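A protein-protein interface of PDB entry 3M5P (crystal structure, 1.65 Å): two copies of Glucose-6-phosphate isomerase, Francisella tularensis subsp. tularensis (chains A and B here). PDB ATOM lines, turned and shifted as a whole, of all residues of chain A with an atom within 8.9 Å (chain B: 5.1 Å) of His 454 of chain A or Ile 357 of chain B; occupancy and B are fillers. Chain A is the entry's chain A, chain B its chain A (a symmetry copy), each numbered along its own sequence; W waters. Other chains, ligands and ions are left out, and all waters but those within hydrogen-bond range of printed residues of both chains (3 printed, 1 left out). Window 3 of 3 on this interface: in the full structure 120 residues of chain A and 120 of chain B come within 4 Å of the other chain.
Water W1 lies within hydrogen-bond range of O of Trp 502 of chain B (2.7 Å), NE2 of Gln 429 of chain A (2.8 Å) and O of Lys 455 of chain A (3.3 Å).
Water W3 bridges OD2 of Asp 500 of chain B (2.8 Å) and ND1 of His 454 of chain A (2.9 Å).
Water W2 lies within hydrogen-bond range of OD1 of Asp 500 of chain B, N of Trp 502 of chain B and OE1 of Gln 388 of chain A.
Among the printed residues, merely in contact across the chains: His 454 of chain A with Asn 356 of chain B, Ala 453 of chain A with Gly 359 of chain B, His 454 of chain A with Thr 84 of chain B, His 454 of chain A with Val 355 of chain B, His 454 of chain A with Trp 502 of chain B, Gln 384 of chain A with Trp 502 of chain B, His 454 of chain A with Gly 359 of chain B, Lys 455 of chain A with Trp 502 of chain B, Leu 451 of chain A with Thr 84 of chain B, Leu 451 of chain A with Trp 502 of chain B, Gln 388 of chain A with Trp 502 of chain B and Ala 453 of chain A with Val 355 of chain B.
No position is printed for both chains.
Of the 13 pairs that touch across the chains among the printed residues, none has its exchanged pair printed and touching as well.
NE2 of His 454 of chain A is in hydrogen-bond range of O of Ile 357 of chain B.
Hydrophobic or aromatic side chains of chain B that line the printed part of chain A: Val 355 and Trp 502.
Hydrophobic or aromatic side chains of chain A that line the printed part of chain B: Leu 451, Ala 453 and His 454.
Among the printed residues, 13 pairs touch across the chains.
OE1 of Gln 388 of chain A is in hydrogen-bond range of NE2 of Gln 384 of chain A, 2.9 Å away.
The side-chain amide nitrogen (NE2) of Gln 388 of chain A is in hydrogen-bond range of the backbone carbonyl oxygen (O) of Val 456 of chain A (2.9 Å).
The side-chain amide nitrogen of Gln 429 of chain A is in hydrogen-bond range of the backbone carbonyl oxygen of Lys 455 of chain A (3.0 Å).
OG1 of Thr 84 of chain B is in hydrogen-bond range of ND2 of Asn 497 of chain B, 3.3 Å away.
OD1 of Asn 356 of chain B lies within hydrogen-bond range of N of Gly 359 of chain B, 3.1 Å away.
The indole nitrogen (NE1) of Trp 502 of chain B sits close to the side-chain carboxylate (OD2) of Asp 500 of chain B, 3.5 Å away.
His 454 of chain A touches six residues of chain B.
Of chain A, only His 454 comes within 4 Å of Ile 357 of chain B.
Of chain A, only His 454 comes within 4 Å of Asn 356 of chain B.
No residue of chain A comes within 4 Å of Ala 358 of chain B.
Of the printed residues of chain B, Leu 451 of chain A touches Thr 84 and Trp 502.
Printed residues of chain A within 4 Å of Trp 502 of chain B: Gln 384 (3.5 Å), Gln 388 (3.8 Å), Leu 451 (3.8 Å), His 454 (3.5 Å) and Lys 455 (3.8 Å).
Printed residues of chain A within 4 Å of Gly 359 of chain B: Ala 453 and His 454.
Asp 495 of chain B touches none of the printed residues of chain A.
Ala 448 of chain A touches none of the printed residues of chain B.
The nearest printed residue of chain A that does not touch Ile 357 of chain B is Glu 450 of chain A (5.9 Å).
The nearest printed residue of chain A that does not touch Thr 84 of chain B is Glu 450 of chain A (6.0 Å).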
ATOM      1  N   GLN A 384      16.654 -22.475  13.392  1.00  0.00           N
ATOM      2  CA  GLN A 384      17.318 -21.952  12.168  1.00  0.00           C
ATOM      3  C   GLN A 384      18.264 -22.985  11.574  1.00  0.00           C
ATOM      4  O   GLN A 384      18.249 -23.194  10.360  1.00  0.00           O
ATOM      5  CB  GLN A 384      18.033 -20.638  12.471  1.00  0.00           C
ATOM      6  CG  GLN A 384      19.077 -20.204  11.462  1.00  0.00           C
ATOM      7  CD  GLN A 384      18.487 -19.876  10.127  1.00  0.00           C
ATOM      8  OE1 GLN A 384      17.421 -19.238  10.050  1.00  0.00           O
ATOM      9  NE2 GLN A 384      19.212 -20.242   9.047  1.00  0.00           N
ATOM     10  N   HIS A 387      16.570 -26.003  10.071  1.00  0.00           N
ATOM     11  CA  HIS A 387      15.897 -25.680   8.799  1.00  0.00           C
ATOM     12  C   HIS A 387      16.864 -25.370   7.619  1.00  0.00           C
ATOM     13  O   HIS A 387      16.610 -25.779   6.489  1.00  0.00           O
ATOM     14  CB  HIS A 387      14.916 -24.507   8.966  1.00  0.00           C
ATOM     15  CG  HIS A 387      13.738 -24.824   9.822  1.00  0.00           C
ATOM     16  ND1 HIS A 387      12.889 -25.891   9.574  1.00  0.00           N
ATOM     17  CD2 HIS A 387      13.294 -24.240  10.968  1.00  0.00           C
ATOM     18  CE1 HIS A 387      11.946 -25.911  10.503  1.00  0.00           C
ATOM     19  NE2 HIS A 387      12.171 -24.925  11.362  1.00  0.00           N
ATOM     20  N   GLN A 388      17.945 -24.664   7.908  1.00  0.00           N
ATOM     21  CA  GLN A 388      18.873 -24.171   6.889  1.00  0.00           C
ATOM     22  C   GLN A 388      20.324 -24.538   7.058  1.00  0.00           C
ATOM     23  O   GLN A 388      21.157 -24.195   6.212  1.00  0.00           O
ATOM     24  CB  GLN A 388      18.770 -22.656   6.751  1.00  0.00           C
ATOM     25  CG  GLN A 388      17.641 -22.196   5.874  1.00  0.00           C
ATOM     26  CD  GLN A 388      17.630 -20.713   5.578  1.00  0.00           C
ATOM     27  OE1 GLN A 388      18.036 -19.898   6.407  1.00  0.00           O
ATOM     28  NE2 GLN A 388      17.113 -20.345   4.395  1.00  0.00           N
ATOM     29  N   GLN A 429      10.827 -24.855   1.370  1.00  0.00           N
ATOM     30  CA  GLN A 429      10.292 -23.947   0.365  1.00  0.00           C
ATOM     31  C   GLN A 429      11.355 -23.714  -0.692  1.00  0.00           C
ATOM     32  O   GLN A 429      12.513 -23.428  -0.392  1.00  0.00           O
ATOM     33  CB  GLN A 429       9.798 -22.620   0.969  1.00  0.00           C
ATOM     34  CG  GLN A 429      10.839 -21.821   1.776  1.00  0.00           C
ATOM     35  CD  GLN A 429      10.263 -20.539   2.436  1.00  0.00           C
ATOM     36  OE1 GLN A 429       9.043 -20.341   2.469  1.00  0.00           O
ATOM     37  NE2 GLN A 429      11.156 -19.676   2.968  1.00  0.00           N
ATOM     38  N   TYR A 431      13.167 -22.343  -4.371  1.00  0.00           N
ATOM     39  CA  TYR A 431      13.549 -21.088  -4.978  1.00  0.00           C
ATOM     40  C   TYR A 431      12.373 -20.447  -5.709  1.00  0.00           C
ATOM     41  O   TYR A 431      12.090 -19.262  -5.506  1.00  0.00           O
ATOM     42  CB  TYR A 431      14.720 -21.318  -5.938  1.00  0.00           C
ATOM     43  CG  TYR A 431      15.234 -20.034  -6.519  1.00  0.00           C
ATOM     44  CD1 TYR A 431      16.346 -19.391  -5.980  1.00  0.00           C
ATOM     45  CD2 TYR A 431      14.596 -19.444  -7.610  1.00  0.00           C
ATOM     46  CE1 TYR A 431      16.810 -18.184  -6.527  1.00  0.00           C
ATOM     47  CE2 TYR A 431      15.033 -18.260  -8.128  1.00  0.00           C
ATOM     48  CZ  TYR A 431      16.141 -17.623  -7.593  1.00  0.00           C
ATOM     49  OH  TYR A 431      16.566 -16.435  -8.182  1.00  0.00           O
ATOM     50  N   VAL A 434       9.760 -19.132  -3.278  1.00  0.00           N
ATOM     51  CA  VAL A 434      10.279 -17.958  -2.584  1.00  0.00           C
ATOM     52  C   VAL A 434      10.344 -16.729  -3.484  1.00  0.00           C
ATOM     53  O   VAL A 434       9.943 -15.615  -3.086  1.00  0.00           O
ATOM     54  CB  VAL A 434      11.674 -18.266  -1.986  1.00  0.00           C
ATOM     55  CG1 VAL A 434      12.399 -16.963  -1.623  1.00  0.00           C
ATOM     56  CG2 VAL A 434      11.501 -19.220  -0.787  1.00  0.00           C
ATOM     57  N   LEU A 438       8.404 -13.210  -3.107  1.00  0.00           N
ATOM     58  CA  LEU A 438       9.097 -11.914  -2.973  1.00  0.00           C
ATOM     59  C   LEU A 438       8.572 -10.886  -3.962  1.00  0.00           C
ATOM     60  O   LEU A 438       8.442  -9.693  -3.638  1.00  0.00           O
ATOM     61  CB  LEU A 438      10.602 -12.078  -3.163  1.00  0.00           C
ATOM     62  CG  LEU A 438      11.354 -12.780  -2.036  1.00  0.00           C
ATOM     63  CD1 LEU A 438      12.851 -12.945  -2.381  1.00  0.00           C
ATOM     64  CD2 LEU A 438      11.153 -11.997  -0.742  1.00  0.00           C
ATOM     65  N   GLN A 447      16.076  -7.310  -6.837  1.00  0.00           N
ATOM     66  CA  GLN A 447      16.034  -7.585  -5.408  1.00  0.00           C
ATOM     67  C   GLN A 447      15.573  -9.016  -5.096  1.00  0.00           C
ATOM     68  O   GLN A 447      16.162  -9.672  -4.221  1.00  0.00           O
ATOM     69  CB  GLN A 447      15.109  -6.602  -4.705  1.00  0.00           C
ATOM     70  CG  GLN A 447      15.531  -5.139  -4.812  1.00  0.00           C
ATOM     71  CD  GLN A 447      14.377  -4.207  -4.419  1.00  0.00           C
ATOM     72  OE1 GLN A 447      13.231  -4.407  -4.833  1.00  0.00           O
ATOM     73  NE2 GLN A 447      14.672  -3.220  -3.597  1.00  0.00           N
ATOM     74  N   ALA A 448      14.489  -9.458  -5.747  1.00  0.00           N
ATOM     75  CA  ALA A 448      13.972 -10.823  -5.543  1.00  0.00           C
ATOM     76  C   ALA A 448      15.038 -11.858  -5.911  1.00  0.00           C
ATOM     77  O   ALA A 448      15.285 -12.800  -5.152  1.00  0.00           O
ATOM     78  CB  ALA A 448      12.682 -11.049  -6.350  1.00  0.00           C
ATOM     79  N   LYS A 449      15.727 -11.648  -7.030  1.00  0.00           N
ATOM     80  CA  LYS A 449      16.759 -12.579  -7.475  1.00  0.00           C
ATOM     81  C   LYS A 449      17.947 -12.621  -6.508  1.00  0.00           C
ATOM     82  O   LYS A 449      18.513 -13.683  -6.270  1.00  0.00           O
ATOM     83  CB  LYS A 449      17.239 -12.217  -8.884  1.00  0.00           C
ATOM     84  CG  LYS A 449      18.341 -13.130  -9.396  1.00  0.00           C
ATOM     85  CD  LYS A 449      18.936 -12.629 -10.715  1.00  0.00           C
ATOM     86  CE  LYS A 449      20.379 -13.128 -10.849  1.00  0.00           C
ATOM     87  NZ  LYS A 449      20.532 -14.505 -10.268  1.00  0.00           N
ATOM     88  N   GLU A 450      18.312 -11.468  -5.942  1.00  0.00           N
ATOM     89  CA  GLU A 450      19.431 -11.385  -5.001  1.00  0.00           C
ATOM     90  C   GLU A 450      19.129 -12.080  -3.676  1.00  0.00           C
ATOM     91  O   GLU A 450      20.025 -12.674  -3.047  1.00  0.00           O
ATOM     92  CB  GLU A 450      19.747  -9.924  -4.727  1.00  0.00           C
ATOM     93  CG  GLU A 450      21.108  -9.673  -4.139  1.00  0.00           C
ATOM     94  CD  GLU A 450      21.704  -8.390  -4.677  1.00  0.00           C
ATOM     95  OE1 GLU A 450      22.134  -8.402  -5.851  1.00  0.00           O
ATOM     96  OE2 GLU A 450      21.724  -7.374  -3.941  1.00  0.00           O
ATOM     97  N   LEU A 451      17.876 -12.006  -3.239  1.00  0.00           N
ATOM     98  CA  LEU A 451      17.504 -12.537  -1.922  1.00  0.00           C
ATOM     99  C   LEU A 451      17.049 -14.000  -1.888  1.00  0.00           C
ATOM    100  O   LEU A 451      17.285 -14.701  -0.882  1.00  0.00           O
ATOM    101  CB  LEU A 451      16.402 -11.654  -1.322  1.00  0.00           C
ATOM    102  CG  LEU A 451      15.891 -11.974   0.094  1.00  0.00           C
ATOM    103  CD1 LEU A 451      17.045 -12.046   1.133  1.00  0.00           C
ATOM    104  CD2 LEU A 451      14.821 -10.923   0.500  1.00  0.00           C
ATOM    105  N   ALA A 452      16.404 -14.458  -2.972  1.00  0.00           N
ATOM    106  CA  ALA A 452      15.638 -15.698  -2.932  1.00  0.00           C
ATOM    107  C   ALA A 452      16.445 -16.896  -2.451  1.00  0.00           C
ATOM    108  O   ALA A 452      15.937 -17.665  -1.658  1.00  0.00           O
ATOM    109  CB  ALA A 452      15.022 -16.027  -4.274  1.00  0.00           C
ATOM    110  N   ALA A 453      17.676 -17.044  -2.944  1.00  0.00           N
ATOM    111  CA  ALA A 453      18.497 -18.193  -2.578  1.00  0.00           C
ATOM    112  C   ALA A 453      18.686 -18.274  -1.084  1.00  0.00           C
ATOM    113  O   ALA A 453      18.810 -19.380  -0.529  1.00  0.00           O
ATOM    114  CB  ALA A 453      19.874 -18.159  -3.269  1.00  0.00           C
ATOM    115  N   HIS A 454      18.739 -17.112  -0.435  1.00  0.00           N
ATOM    116  CA  HIS A 454      18.981 -17.050   1.023  1.00  0.00           C
ATOM    117  C   HIS A 454      17.776 -17.486   1.843  1.00  0.00           C
ATOM    118  O   HIS A 454      17.928 -17.846   2.998  1.00  0.00           O
ATOM    119  CB  HIS A 454      19.367 -15.626   1.395  1.00  0.00           C
ATOM    120  CG  HIS A 454      20.655 -15.224   0.815  1.00  0.00           C
ATOM    121  ND1 HIS A 454      21.865 -15.581   1.374  1.00  0.00           N
ATOM    122  CD2 HIS A 454      20.933 -14.572  -0.333  1.00  0.00           C
ATOM    123  CE1 HIS A 454      22.836 -15.140   0.589  1.00  0.00           C
ATOM    124  NE2 HIS A 454      22.293 -14.511  -0.442  1.00  0.00           N
ATOM    125  N   LYS A 455      16.588 -17.471   1.236  1.00  0.00           N
ATOM    126  CA  LYS A 455      15.359 -17.877   1.879  1.00  0.00           C
ATOM    127  C   LYS A 455      14.947 -19.317   1.559  1.00  0.00           C
ATOM    128  O   LYS A 455      14.029 -19.825   2.173  1.00  0.00           O
ATOM    129  CB  LYS A 455      14.212 -16.919   1.510  1.00  0.00           C
ATOM    130  CG  LYS A 455      14.455 -15.486   1.973  1.00  0.00           C
ATOM    131  CD  LYS A 455      13.268 -14.559   1.752  1.00  0.00           C
ATOM    132  CE  LYS A 455      12.153 -14.867   2.709  1.00  0.00           C
ATOM    133  NZ  LYS A 455      11.069 -13.822   2.635  1.00  0.00           N
ATOM    134  N   VAL A 456      15.629 -19.973   0.623  1.00  0.00           N
ATOM    135  CA  VAL A 456      15.302 -21.346   0.281  1.00  0.00           C
ATOM    136  C   VAL A 456      15.536 -22.234   1.494  1.00  0.00           C
ATOM    137  O   VAL A 456      16.545 -22.121   2.186  1.00  0.00           O
ATOM    138  CB  VAL A 456      16.123 -21.836  -0.930  1.00  0.00           C
ATOM    139  CG1 VAL A 456      16.054 -23.375  -1.069  1.00  0.00           C
ATOM    140  CG2 VAL A 456      15.645 -21.074  -2.184  1.00  0.00           C
ATOM    141  N   ILE A 457      14.561 -23.084   1.770  1.00  0.00           N
ATOM    142  CA  ILE A 457      14.657 -24.051   2.875  1.00  0.00           C
ATOM    143  C   ILE A 457      14.578 -25.429   2.259  1.00  0.00           C
ATOM    144  O   ILE A 457      13.566 -25.774   1.650  1.00  0.00           O
ATOM    145  CB  ILE A 457      13.542 -23.817   3.876  1.00  0.00           C
ATOM    146  CG1 ILE A 457      13.705 -22.407   4.503  1.00  0.00           C
ATOM    147  CG2 ILE A 457      13.581 -24.862   4.984  1.00  0.00           C
ATOM    148  CD1 ILE A 457      12.513 -21.951   5.391  1.00  0.00           C
ATOM    149  N   PRO A 458      15.654 -26.219   2.370  1.00  0.00           N
ATOM    150  CA  PRO A 458      15.688 -27.418   1.519  1.00  0.00           C
ATOM    151  C   PRO A 458      14.555 -28.415   1.772  1.00  0.00           C
ATOM    152  O   PRO A 458      14.055 -29.069   0.849  1.00  0.00           O
ATOM    153  CB  PRO A 458      17.021 -28.082   1.890  1.00  0.00           C
ATOM    154  CG  PRO A 458      17.728 -27.187   2.817  1.00  0.00           C
ATOM    155  CD  PRO A 458      16.931 -25.965   3.072  1.00  0.00           C
ATOM    156  N   SER B  83      24.354  -8.789   4.675  1.00  0.00           N
ATOM    157  CA  SER B  83      24.224  -8.403   3.291  1.00  0.00           C
ATOM    158  C   SER B  83      22.911  -8.823   2.686  1.00  0.00           C
ATOM    159  O   SER B  83      22.542  -8.294   1.639  1.00  0.00           O
ATOM    160  CB  SER B  83      25.382  -8.938   2.493  1.00  0.00           C
ATOM    161  OG  SER B  83      25.500 -10.290   2.701  1.00  0.00           O
ATOM    162  N   THR B  84      22.197  -9.760   3.306  1.00  0.00           N
ATOM    163  CA  THR B  84      20.897 -10.144   2.771  1.00  0.00           C
ATOM    164  C   THR B  84      19.790  -9.184   3.214  1.00  0.00           C
ATOM    165  O   THR B  84      18.801  -9.004   2.509  1.00  0.00           O
ATOM    166  CB  THR B  84      20.519 -11.586   3.146  1.00  0.00           C
ATOM    167  OG1 THR B  84      20.281 -11.682   4.567  1.00  0.00           O
ATOM    168  CG2 THR B  84      21.624 -12.558   2.696  1.00  0.00           C
ATOM    169  N   VAL B 355      23.947 -21.548   2.299  1.00  0.00           N
ATOM    170  CA  VAL B 355      24.411 -20.753   1.173  1.00  0.00           C
ATOM    171  C   VAL B 355      25.427 -19.703   1.598  1.00  0.00           C
ATOM    172  O   VAL B 355      25.402 -19.246   2.717  1.00  0.00           O
ATOM    173  CB  VAL B 355      23.263 -20.056   0.401  1.00  0.00           C
ATOM    174  CG1 VAL B 355      22.289 -21.062  -0.197  1.00  0.00           C
ATOM    175  CG2 VAL B 355      22.561 -19.005   1.213  1.00  0.00           C
ATOM    176  N   ASN B 356      26.335 -19.358   0.685  1.00  0.00           N
ATOM    177  CA  ASN B 356      27.303 -18.290   0.922  1.00  0.00           C
ATOM    178  C   ASN B 356      26.687 -16.918   0.667  1.00  0.00           C
ATOM    179  O   ASN B 356      25.486 -16.821   0.327  1.00  0.00           O
ATOM    180  CB  ASN B 356      28.611 -18.535   0.137  1.00  0.00           C
ATOM    181  CG  ASN B 356      28.412 -18.559  -1.353  1.00  0.00           C
ATOM    182  OD1 ASN B 356      27.406 -18.036  -1.867  1.00  0.00           O
ATOM    183  ND2 ASN B 356      29.393 -19.145  -2.076  1.00  0.00           N
ATOM    184  N   ILE B 357      27.496 -15.872   0.830  1.00  0.00           N
ATOM    185  CA  ILE B 357      27.059 -14.485   0.665  1.00  0.00           C
ATOM    186  C   ILE B 357      26.428 -14.253  -0.703  1.00  0.00           C
ATOM    187  O   ILE B 357      25.462 -13.469  -0.828  1.00  0.00           O
ATOM    188  CB  ILE B 357      28.278 -13.541   0.914  1.00  0.00           C
ATOM    189  CG1 ILE B 357      28.600 -13.559   2.415  1.00  0.00           C
ATOM    190  CG2 ILE B 357      28.021 -12.100   0.435  1.00  0.00           C
ATOM    191  CD1 ILE B 357      27.483 -13.177   3.241  1.00  0.00           C
ATOM    192  N   ALA B 358      26.975 -14.927  -1.724  1.00  0.00           N
ATOM    193  CA  ALA B 358      26.476 -14.841  -3.098  1.00  0.00           C
ATOM    194  C   ALA B 358      25.210 -15.653  -3.369  1.00  0.00           C
ATOM    195  O   ALA B 358      24.665 -15.585  -4.466  1.00  0.00           O
ATOM    196  CB  ALA B 358      27.594 -15.250  -4.091  1.00  0.00           C
ATOM    197  N   GLY B 359      24.761 -16.443  -2.405  1.00  0.00           N
ATOM    198  CA  GLY B 359      23.576 -17.267  -2.556  1.00  0.00           C
ATOM    199  C   GLY B 359      23.822 -18.662  -3.115  1.00  0.00           C
ATOM    200  O   GLY B 359      22.884 -19.365  -3.451  1.00  0.00           O
ATOM    201  N   ASP B 495      32.426 -17.846   4.531  1.00  0.00           N
ATOM    202  CA  ASP B 495      31.819 -16.971   3.531  1.00  0.00           C
ATOM    203  C   ASP B 495      30.297 -16.994   3.586  1.00  0.00           C
ATOM    204  O   ASP B 495      29.619 -16.958   2.551  1.00  0.00           O
ATOM    205  CB  ASP B 495      32.317 -17.374   2.139  1.00  0.00           C
ATOM    206  CG  ASP B 495      32.013 -16.356   1.083  1.00  0.00           C
ATOM    207  OD1 ASP B 495      32.018 -15.159   1.398  1.00  0.00           O
ATOM    208  OD2 ASP B 495      31.816 -16.778  -0.092  1.00  0.00           O
ATOM    209  N   ILE B 496      29.756 -17.036   4.794  1.00  0.00           N
ATOM    210  CA  ILE B 496      28.297 -16.998   5.019  1.00  0.00           C
ATOM    211  C   ILE B 496      27.893 -15.704   5.711  1.00  0.00           C
ATOM    212  O   ILE B 496      28.768 -14.970   6.242  1.00  0.00           O
ATOM    213  CB  ILE B 496      27.779 -18.215   5.826  1.00  0.00           C
ATOM    214  CG1 ILE B 496      28.428 -18.291   7.222  1.00  0.00           C
ATOM    215  CG2 ILE B 496      28.008 -19.540   5.037  1.00  0.00           C
ATOM    216  CD1 ILE B 496      27.809 -19.368   8.185  1.00  0.00           C
ATOM    217  N   ASN B 497      26.587 -15.449   5.751  1.00  0.00           N
ATOM    218  CA  ASN B 497      26.034 -14.328   6.514  1.00  0.00           C
ATOM    219  C   ASN B 497      25.602 -14.798   7.894  1.00  0.00           C
ATOM    220  O   ASN B 497      24.583 -15.455   8.005  1.00  0.00           O
ATOM    221  CB  ASN B 497      24.817 -13.709   5.790  1.00  0.00           C
ATOM    222  CG  ASN B 497      24.312 -12.439   6.483  1.00  0.00           C
ATOM    223  OD1 ASN B 497      24.967 -11.923   7.395  1.00  0.00           O
ATOM    224  ND2 ASN B 497      23.160 -11.938   6.058  1.00  0.00           N
ATOM    225  N   ASP B 500      21.716 -12.916   9.453  1.00  0.00           N
ATOM    226  CA  ASP B 500      20.308 -13.125   9.073  1.00  0.00           C
ATOM    227  C   ASP B 500      19.780 -14.440   9.704  1.00  0.00           C
ATOM    228  O   ASP B 500      20.513 -15.163  10.412  1.00  0.00           O
ATOM    229  CB  ASP B 500      20.118 -13.084   7.536  1.00  0.00           C
ATOM    230  CG  ASP B 500      20.904 -14.162   6.778  1.00  0.00           C
ATOM    231  OD1 ASP B 500      21.297 -15.158   7.411  1.00  0.00           O
ATOM    232  OD2 ASP B 500      21.072 -14.003   5.532  1.00  0.00           O
ATOM    233  N   TRP B 502      16.747 -16.462   7.959  1.00  0.00           N
ATOM    234  CA  TRP B 502      15.605 -16.629   7.088  1.00  0.00           C
ATOM    235  C   TRP B 502      14.893 -17.981   7.298  1.00  0.00           C
ATOM    236  O   TRP B 502      13.716 -18.166   6.911  1.00  0.00           O
ATOM    237  CB  TRP B 502      16.062 -16.484   5.629  1.00  0.00           C
ATOM    238  CG  TRP B 502      16.501 -15.124   5.276  1.00  0.00           C
ATOM    239  CD1 TRP B 502      17.766 -14.731   4.925  1.00  0.00           C
ATOM    240  CD2 TRP B 502      15.701 -13.959   5.244  1.00  0.00           C
ATOM    241  NE1 TRP B 502      17.787 -13.383   4.672  1.00  0.00           N
ATOM    242  CE2 TRP B 502      16.537 -12.883   4.860  1.00  0.00           C
ATOM    243  CE3 TRP B 502      14.364 -13.701   5.522  1.00  0.00           C
ATOM    244  CZ2 TRP B 502      16.064 -11.570   4.745  1.00  0.00           C
ATOM    245  CZ3 TRP B 502      13.905 -12.411   5.403  1.00  0.00           C
ATOM    246  CH2 TRP B 502      14.748 -11.363   4.990  1.00  0.00           C
HETATM  247  O   HOH W   1      12.696 -17.905   4.444  1.00  0.00           O
HETATM  248  O   HOH W   2      19.320 -17.109   6.956  1.00  0.00           O
HETATM  249  O   HOH W   3      22.095 -16.200   4.153  1.00  0.00           O
